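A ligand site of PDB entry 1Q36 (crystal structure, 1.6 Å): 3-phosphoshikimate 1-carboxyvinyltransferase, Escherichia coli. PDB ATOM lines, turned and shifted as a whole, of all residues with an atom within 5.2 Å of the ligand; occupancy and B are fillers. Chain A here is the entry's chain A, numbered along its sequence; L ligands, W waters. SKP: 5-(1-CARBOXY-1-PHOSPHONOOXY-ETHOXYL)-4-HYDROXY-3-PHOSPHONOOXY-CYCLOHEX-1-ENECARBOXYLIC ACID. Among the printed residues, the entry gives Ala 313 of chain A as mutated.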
ATOM      1  N   LYS A  22      22.556   5.675 -20.714  1.00  0.00           N
ATOM      2  CA  LYS A  22      21.909   4.357 -20.519  1.00  0.00           C
ATOM      3  C   LYS A  22      20.616   4.227 -21.343  1.00  0.00           C
ATOM      4  O   LYS A  22      20.398   3.166 -21.987  1.00  0.00           O
ATOM      5  CB  LYS A  22      21.610   4.153 -18.993  1.00  0.00           C
ATOM      6  CG  LYS A  22      20.861   2.811 -18.722  1.00  0.00           C
ATOM      7  CD  LYS A  22      19.368   3.077 -18.408  1.00  0.00           C
ATOM      8  CE  LYS A  22      19.217   3.575 -16.927  1.00  0.00           C
ATOM      9  NZ  LYS A  22      17.867   4.070 -16.602  1.00  0.00           N
ATOM     10  N   SER A  23      19.791   5.257 -21.321  1.00  0.00           N
ATOM     11  CA  SER A  23      18.526   5.242 -22.059  1.00  0.00           C
ATOM     12  C   SER A  23      18.752   5.058 -23.563  1.00  0.00           C
ATOM     13  O   SER A  23      18.056   4.277 -24.210  1.00  0.00           O
ATOM     14  CB  SER A  23      17.770   6.546 -21.824  1.00  0.00           C
ATOM     15  OG  SER A  23      17.400   6.614 -20.439  1.00  0.00           O
ATOM     16  N   ARG A  27      18.166   1.269 -25.915  1.00  0.00           N
ATOM     17  CA  ARG A  27      17.256   1.329 -27.064  1.00  0.00           C
ATOM     18  C   ARG A  27      18.055   1.014 -28.339  1.00  0.00           C
ATOM     19  O   ARG A  27      17.599   0.270 -29.202  1.00  0.00           O
ATOM     20  CB  ARG A  27      16.662   2.750 -27.206  1.00  0.00           C
ATOM     21  CG  ARG A  27      15.530   3.037 -26.216  1.00  0.00           C
ATOM     22  CD  ARG A  27      15.357   4.573 -26.192  1.00  0.00           C
ATOM     23  NE  ARG A  27      14.229   5.038 -25.424  1.00  0.00           N
ATOM     24  CZ  ARG A  27      14.177   5.136 -24.093  1.00  0.00           C
ATOM     25  NH1 ARG A  27      13.075   5.614 -23.506  1.00  0.00           N
ATOM     26  NH2 ARG A  27      15.220   4.738 -23.331  1.00  0.00           N
ATOM     27  N   ASP A  49      23.133  -2.155 -16.439  1.00  0.00           N
ATOM     28  CA  ASP A  49      21.942  -2.220 -17.272  1.00  0.00           C
ATOM     29  C   ASP A  49      22.242  -2.570 -18.707  1.00  0.00           C
ATOM     30  O   ASP A  49      21.463  -3.285 -19.331  1.00  0.00           O
ATOM     31  CB  ASP A  49      21.154  -0.932 -17.248  1.00  0.00           C
ATOM     32  CG  ASP A  49      20.393  -0.702 -15.932  1.00  0.00           C
ATOM     33  OD1 ASP A  49      20.363  -1.600 -15.067  1.00  0.00           O
ATOM     34  OD2 ASP A  49      19.780   0.403 -15.829  1.00  0.00           O
ATOM     35  N   ASN A  94      18.222  -5.204 -12.776  1.00  0.00           N
ATOM     36  CA  ASN A  94      17.103  -4.306 -12.365  1.00  0.00           C
ATOM     37  C   ASN A  94      16.974  -3.252 -13.470  1.00  0.00           C
ATOM     38  O   ASN A  94      16.601  -2.116 -13.219  1.00  0.00           O
ATOM     39  CB  ASN A  94      17.336  -3.619 -11.009  1.00  0.00           C
ATOM     40  CG  ASN A  94      16.033  -3.040 -10.427  1.00  0.00           C
ATOM     41  OD1 ASN A  94      14.929  -3.344 -10.903  1.00  0.00           O
ATOM     42  ND2 ASN A  94      16.147  -2.265  -9.336  1.00  0.00           N
ATOM     43  N   ALA A  95      17.211  -3.699 -14.714  1.00  0.00           N
ATOM     44  CA  ALA A  95      17.181  -2.777 -15.869  1.00  0.00           C
ATOM     45  C   ALA A  95      15.811  -2.598 -16.477  1.00  0.00           C
ATOM     46  O   ALA A  95      15.335  -3.462 -17.223  1.00  0.00           O
ATOM     47  CB  ALA A  95      18.169  -3.277 -16.927  1.00  0.00           C
ATOM     48  N   GLY A  96      15.148  -1.484 -16.166  1.00  0.00           N
ATOM     49  CA  GLY A  96      13.858  -1.269 -16.779  1.00  0.00           C
ATOM     50  C   GLY A  96      13.944  -1.160 -18.297  1.00  0.00           C
ATOM     51  O   GLY A  96      13.023  -1.596 -19.009  1.00  0.00           O
ATOM     52  N   THR A  97      15.046  -0.609 -18.787  1.00  0.00           N
ATOM     53  CA  THR A  97      15.184  -0.415 -20.233  1.00  0.00           C
ATOM     54  C   THR A  97      15.506  -1.710 -20.934  1.00  0.00           C
ATOM     55  O   THR A  97      15.621  -1.707 -22.161  1.00  0.00           O
ATOM     56  CB  THR A  97      16.242   0.633 -20.604  1.00  0.00           C
ATOM     57  OG1 THR A  97      17.509   0.295 -20.041  1.00  0.00           O
ATOM     58  CG2 THR A  97      15.804   1.983 -20.079  1.00  0.00           C
ATOM     59  N   ARG A 100      11.286  -3.775 -19.780  1.00  0.00           N
ATOM     60  CA  ARG A 100      10.060  -3.321 -20.425  1.00  0.00           C
ATOM     61  C   ARG A 100      10.157  -3.495 -21.945  1.00  0.00           C
ATOM     62  O   ARG A 100       9.280  -4.129 -22.540  1.00  0.00           O
ATOM     63  CB  ARG A 100       9.715  -1.876 -20.015  1.00  0.00           C
ATOM     64  CG  ARG A 100       9.004  -1.724 -18.638  1.00  0.00           C
ATOM     65  CD  ARG A 100       9.884  -2.152 -17.449  1.00  0.00           C
ATOM     66  NE  ARG A 100       9.176  -1.944 -16.165  1.00  0.00           N
ATOM     67  CZ  ARG A 100       9.258  -0.812 -15.458  1.00  0.00           C
ATOM     68  NH1 ARG A 100       8.587  -0.684 -14.322  1.00  0.00           N
ATOM     69  NH2 ARG A 100      10.009   0.185 -15.891  1.00  0.00           N
ATOM     70  N   ARG A 124       8.770  -4.131  -9.357  1.00  0.00           N
ATOM     71  CA  ARG A 124       8.589  -2.939 -10.219  1.00  0.00           C
ATOM     72  C   ARG A 124       7.468  -3.332 -11.169  1.00  0.00           C
ATOM     73  O   ARG A 124       7.543  -4.341 -11.889  1.00  0.00           O
ATOM     74  CB  ARG A 124       9.888  -2.568 -10.934  1.00  0.00           C
ATOM     75  CG  ARG A 124      10.940  -2.019  -9.934  1.00  0.00           C
ATOM     76  CD  ARG A 124      12.180  -1.556 -10.607  1.00  0.00           C
ATOM     77  NE  ARG A 124      11.912  -0.423 -11.484  1.00  0.00           N
ATOM     78  CZ  ARG A 124      12.792   0.061 -12.365  1.00  0.00           C
ATOM     79  NH1 ARG A 124      12.430   1.105 -13.115  1.00  0.00           N
ATOM     80  NH2 ARG A 124      14.010  -0.477 -12.494  1.00  0.00           N
ATOM     81  N   VAL A 168       1.998   5.628 -14.824  1.00  0.00           N
ATOM     82  CA  VAL A 168       3.050   5.118 -13.939  1.00  0.00           C
ATOM     83  C   VAL A 168       4.464   5.098 -14.534  1.00  0.00           C
ATOM     84  O   VAL A 168       5.468   5.374 -13.851  1.00  0.00           O
ATOM     85  CB  VAL A 168       2.657   3.710 -13.435  1.00  0.00           C
ATOM     86  CG1 VAL A 168       3.797   3.074 -12.652  1.00  0.00           C
ATOM     87  CG2 VAL A 168       1.436   3.838 -12.552  1.00  0.00           C
ATOM     88  N   SER A 169       4.583   4.723 -15.809  1.00  0.00           N
ATOM     89  CA  SER A 169       5.899   4.715 -16.459  1.00  0.00           C
ATOM     90  C   SER A 169       5.725   5.016 -17.939  1.00  0.00           C
ATOM     91  O   SER A 169       4.755   4.557 -18.578  1.00  0.00           O
ATOM     92  CB  SER A 169       6.546   3.317 -16.340  1.00  0.00           C
ATOM     93  OG  SER A 169       7.798   3.328 -16.989  1.00  0.00           O
ATOM     94  N   SER A 170       6.648   5.770 -18.495  1.00  0.00           N
ATOM     95  CA  SER A 170       6.651   6.022 -19.927  1.00  0.00           C
ATOM     96  C   SER A 170       7.262   4.791 -20.621  1.00  0.00           C
ATOM     97  O   SER A 170       7.123   4.629 -21.830  1.00  0.00           O
ATOM     98  CB  SER A 170       7.522   7.237 -20.257  1.00  0.00           C
ATOM     99  OG  SER A 170       8.902   6.980 -20.024  1.00  0.00           O
ATOM    100  N   GLN A 171       7.874   3.887 -19.861  1.00  0.00           N
ATOM    101  CA  GLN A 171       8.511   2.749 -20.498  1.00  0.00           C
ATOM    102  C   GLN A 171       7.585   1.775 -21.166  1.00  0.00           C
ATOM    103  O   GLN A 171       7.972   1.071 -22.077  1.00  0.00           O
ATOM    104  CB  GLN A 171       9.409   1.996 -19.504  1.00  0.00           C
ATOM    105  CG  GLN A 171      10.585   2.856 -19.076  1.00  0.00           C
ATOM    106  CD  GLN A 171      11.613   2.064 -18.285  1.00  0.00           C
ATOM    107  OE1 GLN A 171      11.509   0.856 -18.112  1.00  0.00           O
ATOM    108  NE2 GLN A 171      12.650   2.760 -17.830  1.00  0.00           N
ATOM    109  N   THR A 174       6.962   3.298 -24.484  1.00  0.00           N
ATOM    110  CA  THR A 174       8.177   3.113 -25.240  1.00  0.00           C
ATOM    111  C   THR A 174       8.300   1.700 -25.799  1.00  0.00           C
ATOM    112  O   THR A 174       8.650   1.509 -26.984  1.00  0.00           O
ATOM    113  CB  THR A 174       9.396   3.417 -24.355  1.00  0.00           C
ATOM    114  OG1 THR A 174       9.587   4.834 -24.399  1.00  0.00           O
ATOM    115  CG2 THR A 174      10.669   2.665 -24.823  1.00  0.00           C
ATOM    116  N   VAL A 196       3.365  10.245 -17.866  1.00  0.00           N
ATOM    117  CA  VAL A 196       4.472  10.781 -17.096  1.00  0.00           C
ATOM    118  C   VAL A 196       5.756  10.563 -17.854  1.00  0.00           C
ATOM    119  O   VAL A 196       5.796   9.796 -18.841  1.00  0.00           O
ATOM    120  CB  VAL A 196       4.596  10.068 -15.739  1.00  0.00           C
ATOM    121  CG1 VAL A 196       3.388  10.383 -14.882  1.00  0.00           C
ATOM    122  CG2 VAL A 196       4.741   8.546 -15.941  1.00  0.00           C
ATOM    123  N   SER A 197       6.796  11.261 -17.432  1.00  0.00           N
ATOM    124  CA  SER A 197       8.113  11.106 -18.052  1.00  0.00           C
ATOM    125  C   SER A 197       8.106  11.248 -19.571  1.00  0.00           C
ATOM    126  O   SER A 197       8.838  10.556 -20.276  1.00  0.00           O
ATOM    127  CB  SER A 197       8.664   9.730 -17.656  1.00  0.00           C
ATOM    128  OG  SER A 197       8.917   9.718 -16.249  1.00  0.00           O
ATOM    129  N   TYR A 200      11.024  10.894 -22.311  1.00  0.00           N
ATOM    130  CA  TYR A 200      11.627   9.627 -22.699  1.00  0.00           C
ATOM    131  C   TYR A 200      10.977   9.072 -23.934  1.00  0.00           C
ATOM    132  O   TYR A 200      11.602   8.286 -24.662  1.00  0.00           O
ATOM    133  CB  TYR A 200      11.591   8.600 -21.533  1.00  0.00           C
ATOM    134  CG  TYR A 200      12.546   8.994 -20.444  1.00  0.00           C
ATOM    135  CD1 TYR A 200      12.111   9.722 -19.333  1.00  0.00           C
ATOM    136  CD2 TYR A 200      13.888   8.606 -20.530  1.00  0.00           C
ATOM    137  CE1 TYR A 200      13.002  10.072 -18.314  1.00  0.00           C
ATOM    138  CE2 TYR A 200      14.792   8.943 -19.471  1.00  0.00           C
ATOM    139  CZ  TYR A 200      14.325   9.671 -18.378  1.00  0.00           C
ATOM    140  OH  TYR A 200      15.176   9.898 -17.290  1.00  0.00           O
ATOM    141  N   PRO A 312      12.455  13.217 -13.791  1.00  0.00           N
ATOM    142  CA  PRO A 312      12.413  12.420 -12.571  1.00  0.00           C
ATOM    143  C   PRO A 312      13.761  11.924 -12.061  1.00  0.00           C
ATOM    144  O   PRO A 312      13.957  11.880 -10.835  1.00  0.00           O
ATOM    145  CB  PRO A 312      11.465  11.267 -12.922  1.00  0.00           C
ATOM    146  CG  PRO A 312      11.685  11.089 -14.405  1.00  0.00           C
ATOM    147  CD  PRO A 312      11.713  12.544 -14.891  1.00  0.00           C
ATOM    148  N   ALA A 313      14.678  11.590 -12.964  1.00  0.00           N
ATOM    149  CA  ALA A 313      15.972  11.074 -12.537  1.00  0.00           C
ATOM    150  C   ALA A 313      16.848  12.201 -12.010  1.00  0.00           C
ATOM    151  O   ALA A 313      17.297  12.184 -10.842  1.00  0.00           O
ATOM    152  CB  ALA A 313      16.644  10.381 -13.655  1.00  0.00           C
ATOM    153  N   ASN A 336       6.208   8.551  -9.303  1.00  0.00           N
ATOM    154  CA  ASN A 336       6.855   7.297  -9.710  1.00  0.00           C
ATOM    155  C   ASN A 336       8.267   7.046  -9.220  1.00  0.00           C
ATOM    156  O   ASN A 336       8.868   5.988  -9.510  1.00  0.00           O
ATOM    157  CB  ASN A 336       6.681   7.020 -11.222  1.00  0.00           C
ATOM    158  CG  ASN A 336       7.669   7.746 -12.110  1.00  0.00           C
ATOM    159  OD1 ASN A 336       8.528   8.519 -11.662  1.00  0.00           O
ATOM    160  ND2 ASN A 336       7.555   7.470 -13.408  1.00  0.00           N
ATOM    161  N   LYS A 340      10.632   2.714  -8.548  1.00  0.00           N
ATOM    162  CA  LYS A 340      11.863   2.540  -9.293  1.00  0.00           C
ATOM    163  C   LYS A 340      12.887   1.648  -8.593  1.00  0.00           C
ATOM    164  O   LYS A 340      12.465   0.710  -7.932  1.00  0.00           O
ATOM    165  CB  LYS A 340      12.381   3.918  -9.658  1.00  0.00           C
ATOM    166  CG  LYS A 340      11.608   4.393 -10.928  1.00  0.00           C
ATOM    167  CD  LYS A 340      11.779   5.857 -11.198  1.00  0.00           C
ATOM    168  CE  LYS A 340      11.038   6.138 -12.522  1.00  0.00           C
ATOM    169  NZ  LYS A 340      11.000   7.599 -12.881  1.00  0.00           N
ATOM    170  N   GLU A 341      14.205   1.914  -8.706  1.00  0.00           N
ATOM    171  CA  GLU A 341      15.195   1.022  -8.073  1.00  0.00           C
ATOM    172  C   GLU A 341      14.909   0.802  -6.601  1.00  0.00           C
ATOM    173  O   GLU A 341      15.237  -0.251  -6.049  1.00  0.00           O
ATOM    174  CB  GLU A 341      16.633   1.551  -8.274  1.00  0.00           C
ATOM    175  CG  GLU A 341      17.147   1.437  -9.760  1.00  0.00           C
ATOM    176  CD  GLU A 341      16.666   2.560 -10.730  1.00  0.00           C
ATOM    177  OE1 GLU A 341      15.541   3.136 -10.574  1.00  0.00           O
ATOM    178  OE2 GLU A 341      17.419   2.836 -11.680  1.00  0.00           O
ATOM    179  N   ARG A 344      12.070   5.845  -3.974  1.00  0.00           N
ATOM    180  CA  ARG A 344      12.991   6.968  -3.811  1.00  0.00           C
ATOM    181  C   ARG A 344      12.461   8.112  -2.968  1.00  0.00           C
ATOM    182  O   ARG A 344      13.237   8.882  -2.429  1.00  0.00           O
ATOM    183  CB  ARG A 344      13.430   7.482  -5.194  1.00  0.00           C
ATOM    184  CG  ARG A 344      14.345   6.480  -5.863  1.00  0.00           C
ATOM    185  CD  ARG A 344      14.474   6.783  -7.376  1.00  0.00           C
ATOM    186  NE  ARG A 344      15.705   6.175  -7.900  1.00  0.00           N
ATOM    187  CZ  ARG A 344      16.025   6.112  -9.196  1.00  0.00           C
ATOM    188  NH1 ARG A 344      17.196   5.563  -9.555  1.00  0.00           N
ATOM    189  NH2 ARG A 344      15.194   6.567 -10.138  1.00  0.00           N
ATOM    190  N   HIS A 385      21.765   3.127  -7.539  1.00  0.00           N
ATOM    191  CA  HIS A 385      22.879   3.967  -8.012  1.00  0.00           C
ATOM    192  C   HIS A 385      22.641   5.431  -7.723  1.00  0.00           C
ATOM    193  O   HIS A 385      23.591   6.128  -7.307  1.00  0.00           O
ATOM    194  CB  HIS A 385      23.083   3.792  -9.539  1.00  0.00           C
ATOM    195  CG  HIS A 385      21.840   3.963 -10.356  1.00  0.00           C
ATOM    196  ND1 HIS A 385      21.864   4.586 -11.574  1.00  0.00           N
ATOM    197  CD2 HIS A 385      20.544   3.597 -10.157  1.00  0.00           C
ATOM    198  CE1 HIS A 385      20.649   4.613 -12.097  1.00  0.00           C
ATOM    199  NE2 HIS A 385      19.827   4.015 -11.263  1.00  0.00           N
ATOM    200  N   ARG A 386      21.407   5.932  -7.904  1.00  0.00           N
ATOM    201  CA  ARG A 386      21.215   7.361  -7.713  1.00  0.00           C
ATOM    202  C   ARG A 386      21.259   7.833  -6.275  1.00  0.00           C
ATOM    203  O   ARG A 386      21.567   9.006  -6.004  1.00  0.00           O
ATOM    204  CB  ARG A 386      19.924   7.821  -8.408  1.00  0.00           C
ATOM    205  CG  ARG A 386      19.994   7.558  -9.891  1.00  0.00           C
ATOM    206  CD  ARG A 386      18.964   8.429 -10.668  1.00  0.00           C
ATOM    207  NE  ARG A 386      18.924   7.912 -12.042  1.00  0.00           N
ATOM    208  CZ  ARG A 386      19.873   8.048 -12.951  1.00  0.00           C
ATOM    209  NH1 ARG A 386      19.721   7.473 -14.167  1.00  0.00           N
ATOM    210  NH2 ARG A 386      20.956   8.810 -12.727  1.00  0.00           N
ATOM    211  N   LYS A 411      25.053   0.443 -11.768  1.00  0.00           N
ATOM    212  CA  LYS A 411      23.874   0.248 -12.572  1.00  0.00           C
ATOM    213  C   LYS A 411      23.965   1.119 -13.843  1.00  0.00           C
ATOM    214  O   LYS A 411      23.606   0.651 -14.924  1.00  0.00           O
ATOM    215  CB  LYS A 411      22.572   0.601 -11.823  1.00  0.00           C
ATOM    216  CG  LYS A 411      21.312   0.126 -12.566  1.00  0.00           C
ATOM    217  CD  LYS A 411      20.048   0.191 -11.685  1.00  0.00           C
ATOM    218  CE  LYS A 411      18.758  -0.279 -12.409  1.00  0.00           C
ATOM    219  NZ  LYS A 411      18.363   0.687 -13.465  1.00  0.00           N
ATOM    220  N   THR A 412      24.455   2.346 -13.689  1.00  0.00           N
ATOM    221  CA  THR A 412      24.619   3.245 -14.817  1.00  0.00           C
ATOM    222  C   THR A 412      25.963   3.949 -14.886  1.00  0.00           C
ATOM    223  O   THR A 412      26.265   4.617 -15.872  1.00  0.00           O
ATOM    224  CB  THR A 412      23.548   4.377 -14.814  1.00  0.00           C
ATOM    225  OG1 THR A 412      23.679   5.176 -13.637  1.00  0.00           O
ATOM    226  CG2 THR A 412      22.139   3.830 -14.905  1.00  0.00           C
HETATM  227  C1  SKP L   1      13.721   5.644 -18.785  1.00  0.00           C
HETATM  228  C2  SKP L   1      12.522   6.327 -18.475  1.00  0.00           C
HETATM  229  C3  SKP L   1      12.289   6.745 -17.023  1.00  0.00           C
HETATM  230  C4  SKP L   1      13.625   6.827 -16.195  1.00  0.00           C
HETATM  231  C5  SKP L   1      14.343   5.478 -16.273  1.00  0.00           C
HETATM  232  C6  SKP L   1      14.759   5.324 -17.777  1.00  0.00           C
HETATM  233  C7  SKP L   1      13.954   5.255 -20.220  1.00  0.00           C
HETATM  234  O1  SKP L   1      11.315   5.799 -16.394  1.00  0.00           O
HETATM  235  O2  SKP L   1      13.283   7.161 -14.836  1.00  0.00           O
HETATM  236  O3  SKP L   1      15.519   5.525 -15.463  1.00  0.00           O
HETATM  237  O4  SKP L   1      12.978   4.986 -20.896  1.00  0.00           O
HETATM  238  O5  SKP L   1      15.087   5.238 -20.591  1.00  0.00           O
HETATM  239  P1  SKP L   1       9.787   6.188 -16.124  1.00  0.00           P
HETATM  240  O6  SKP L   1       9.097   6.426 -17.485  1.00  0.00           O
HETATM  241  O7  SKP L   1       9.831   7.479 -15.231  1.00  0.00           O
HETATM  242  O8  SKP L   1       9.232   4.928 -15.439  1.00  0.00           O
HETATM  243  C8  SKP L   1      15.706   4.790 -14.249  1.00  0.00           C
HETATM  244  C9  SKP L   1      14.479   4.738 -13.288  1.00  0.00           C
HETATM  245  C10 SKP L   1      16.879   5.397 -13.543  1.00  0.00           C
HETATM  246  O9  SKP L   1      17.952   5.109 -14.145  1.00  0.00           O
HETATM  247  O10 SKP L   1      16.799   6.137 -12.538  1.00  0.00           O
HETATM  248  P2  SKP L   1      15.327   2.057 -15.281  1.00  0.00           P
HETATM  249  O11 SKP L   1      15.682   0.748 -14.552  1.00  0.00           O
HETATM  250  O12 SKP L   1      15.901   2.052 -16.675  1.00  0.00           O
HETATM  251  O13 SKP L   1      13.784   2.240 -15.272  1.00  0.00           O
HETATM  252  O14 SKP L   1      16.046   3.337 -14.488  1.00  0.00           O
HETATM  253  O   HOH W   1      10.372   5.375 -21.757  1.00  0.00           O
HETATM  254  O   HOH W   2      17.511   0.404 -17.404  1.00  0.00           O
HETATM  255  O   HOH W   3      10.887   2.863 -14.869  1.00  0.00           O
HETATM  256  O   HOH W   4       8.165   4.051 -13.227  1.00  0.00           O
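The backbone NH (N) of Ser 170 is in hydrogen-bond range of an oxygen (O6) of the ligand (2.7 Å).
The side-chain hydroxyl (OG) of Ser 170 sits at hydrogen-bond distance from an oxygen (O6) of the ligand, 2.6 Å away.
The side-chain hydroxyl of Ser 197 is in hydrogen-bond range of an oxygen (O7) of the ligand, 2.6 Å away.
O7 of the ligand lies within salt-bridge range of NZ of Lys 340.
The side-chain hydroxyl (OG) of Ser 169 is in hydrogen-bond range of an oxygen (O8) of the ligand, 2.6 Å away.
NZ of Lys 22 lies within salt-bridge range of O9 of the ligand, at 2.7 Å.
The guanidinium group (NH1) of Arg 27 is in salt-bridge range of an oxygen (O4) of the ligand, 2.7 Å away.
An oxygen (O5) of the ligand sits at hydrogen-bond distance from the side-chain hydroxyl of Ser 23, 2.7 Å away.
NH1 of Arg 124 lies within salt-bridge range of O13 of the ligand, 2.8 Å away.
O11 of the ligand lies within hydrogen-bond range of N of Gly 96 (2.8 Å).
NE of Arg 386 is in salt-bridge range of O10 of the ligand.
An oxygen (O13) of the ligand sits at hydrogen-bond distance from the side-chain amide nitrogen of Gln 171 (2.8 Å).
The side-chain amino group (NZ) of Lys 411 is in salt-bridge range of an oxygen (O11) of the ligand (2.9 Å).
The side-chain amide nitrogen (ND2) of Asn 336 is in hydrogen-bond range of an oxygen (O7) of the ligand, at 2.9 Å.
The guanidinium group (NH2) of Arg 344 lies within salt-bridge range of an oxygen (O10) of the ligand (2.9 Å).
Water W2 lies within hydrogen-bond range of O12 of the ligand (2.4 Å), OG1 of Thr 97 (2.6 Å), OD2 of Asp 49 (2.8 Å) and N of Gly 96 (3.3 Å).
Water W4 lies within hydrogen-bond range of O8 of the ligand, O of Val 168 and ND2 of Asn 336.
Water W1 lies within hydrogen-bond range of an oxygen (O4) of the ligand, the side-chain hydroxyl of Ser 170, the side-chain hydroxyl of Thr 174, the guanidinium group of Arg 27 and the backbone NH of Gln 171.
The backbone carbonyl oxygen (O) of Asn 94 lies close to an oxygen (O11) of the ligand (3.3 Å).
OE2 of Glu 341 lies close to O14 of the ligand, at 3.2 Å.
Ala 95 touches the ligand (C to O11, 3.9 Å).
Thr 97 touches the ligand (CG2 to O5, 3.4 Å).
Tyr 200 touches the ligand (CG to C2, 3.3 Å).
His 385 touches the ligand (CE1 to O9, 3.4 Å).
Hydrophobic or aromatic side chains within 4 Å of the ligand: Tyr 200 and His 385.
Of the 28 residues printed, 20 come within 4 Å of the ligand.
Along chain A the residues within 4 Å of the ligand span positions 22 to 411.
The nearest printed residue that does not touch the ligand is Val 168 (4.1 Å).
The backbone NH (N) of Gln 171 is in hydrogen-bond range of the side-chain hydroxyl (OG) of Ser 169 (2.9 Å).
The guanidinium group of Arg 27 is in hydrogen-bond range of the backbone carbonyl oxygen of Tyr 200 (3.3 Å).
NH2 of Arg 124 lies within hydrogen-bond range of O of Asn 94 (3.2 Å).
The backbone carbonyl oxygen of Gly 96 lies close to the side-chain amide oxygen of Gln 171 (3.0 Å).
The side-chain amino group of Lys 411 sits close to the backbone carbonyl oxygen of Asn 94, 3.3 Å away.
NH1 of Arg 344 sits at hydrogen-bond distance from NE2 of His 385 (3.5 Å).
OE2 of Glu 341 lies within hydrogen-bond range of NE2 of His 385 (2.7 Å).
The side-chain hydroxyl (OG1) of Thr 412 sits at hydrogen-bond distance from a ring nitrogen (ND1) of His 385 (2.8 Å).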
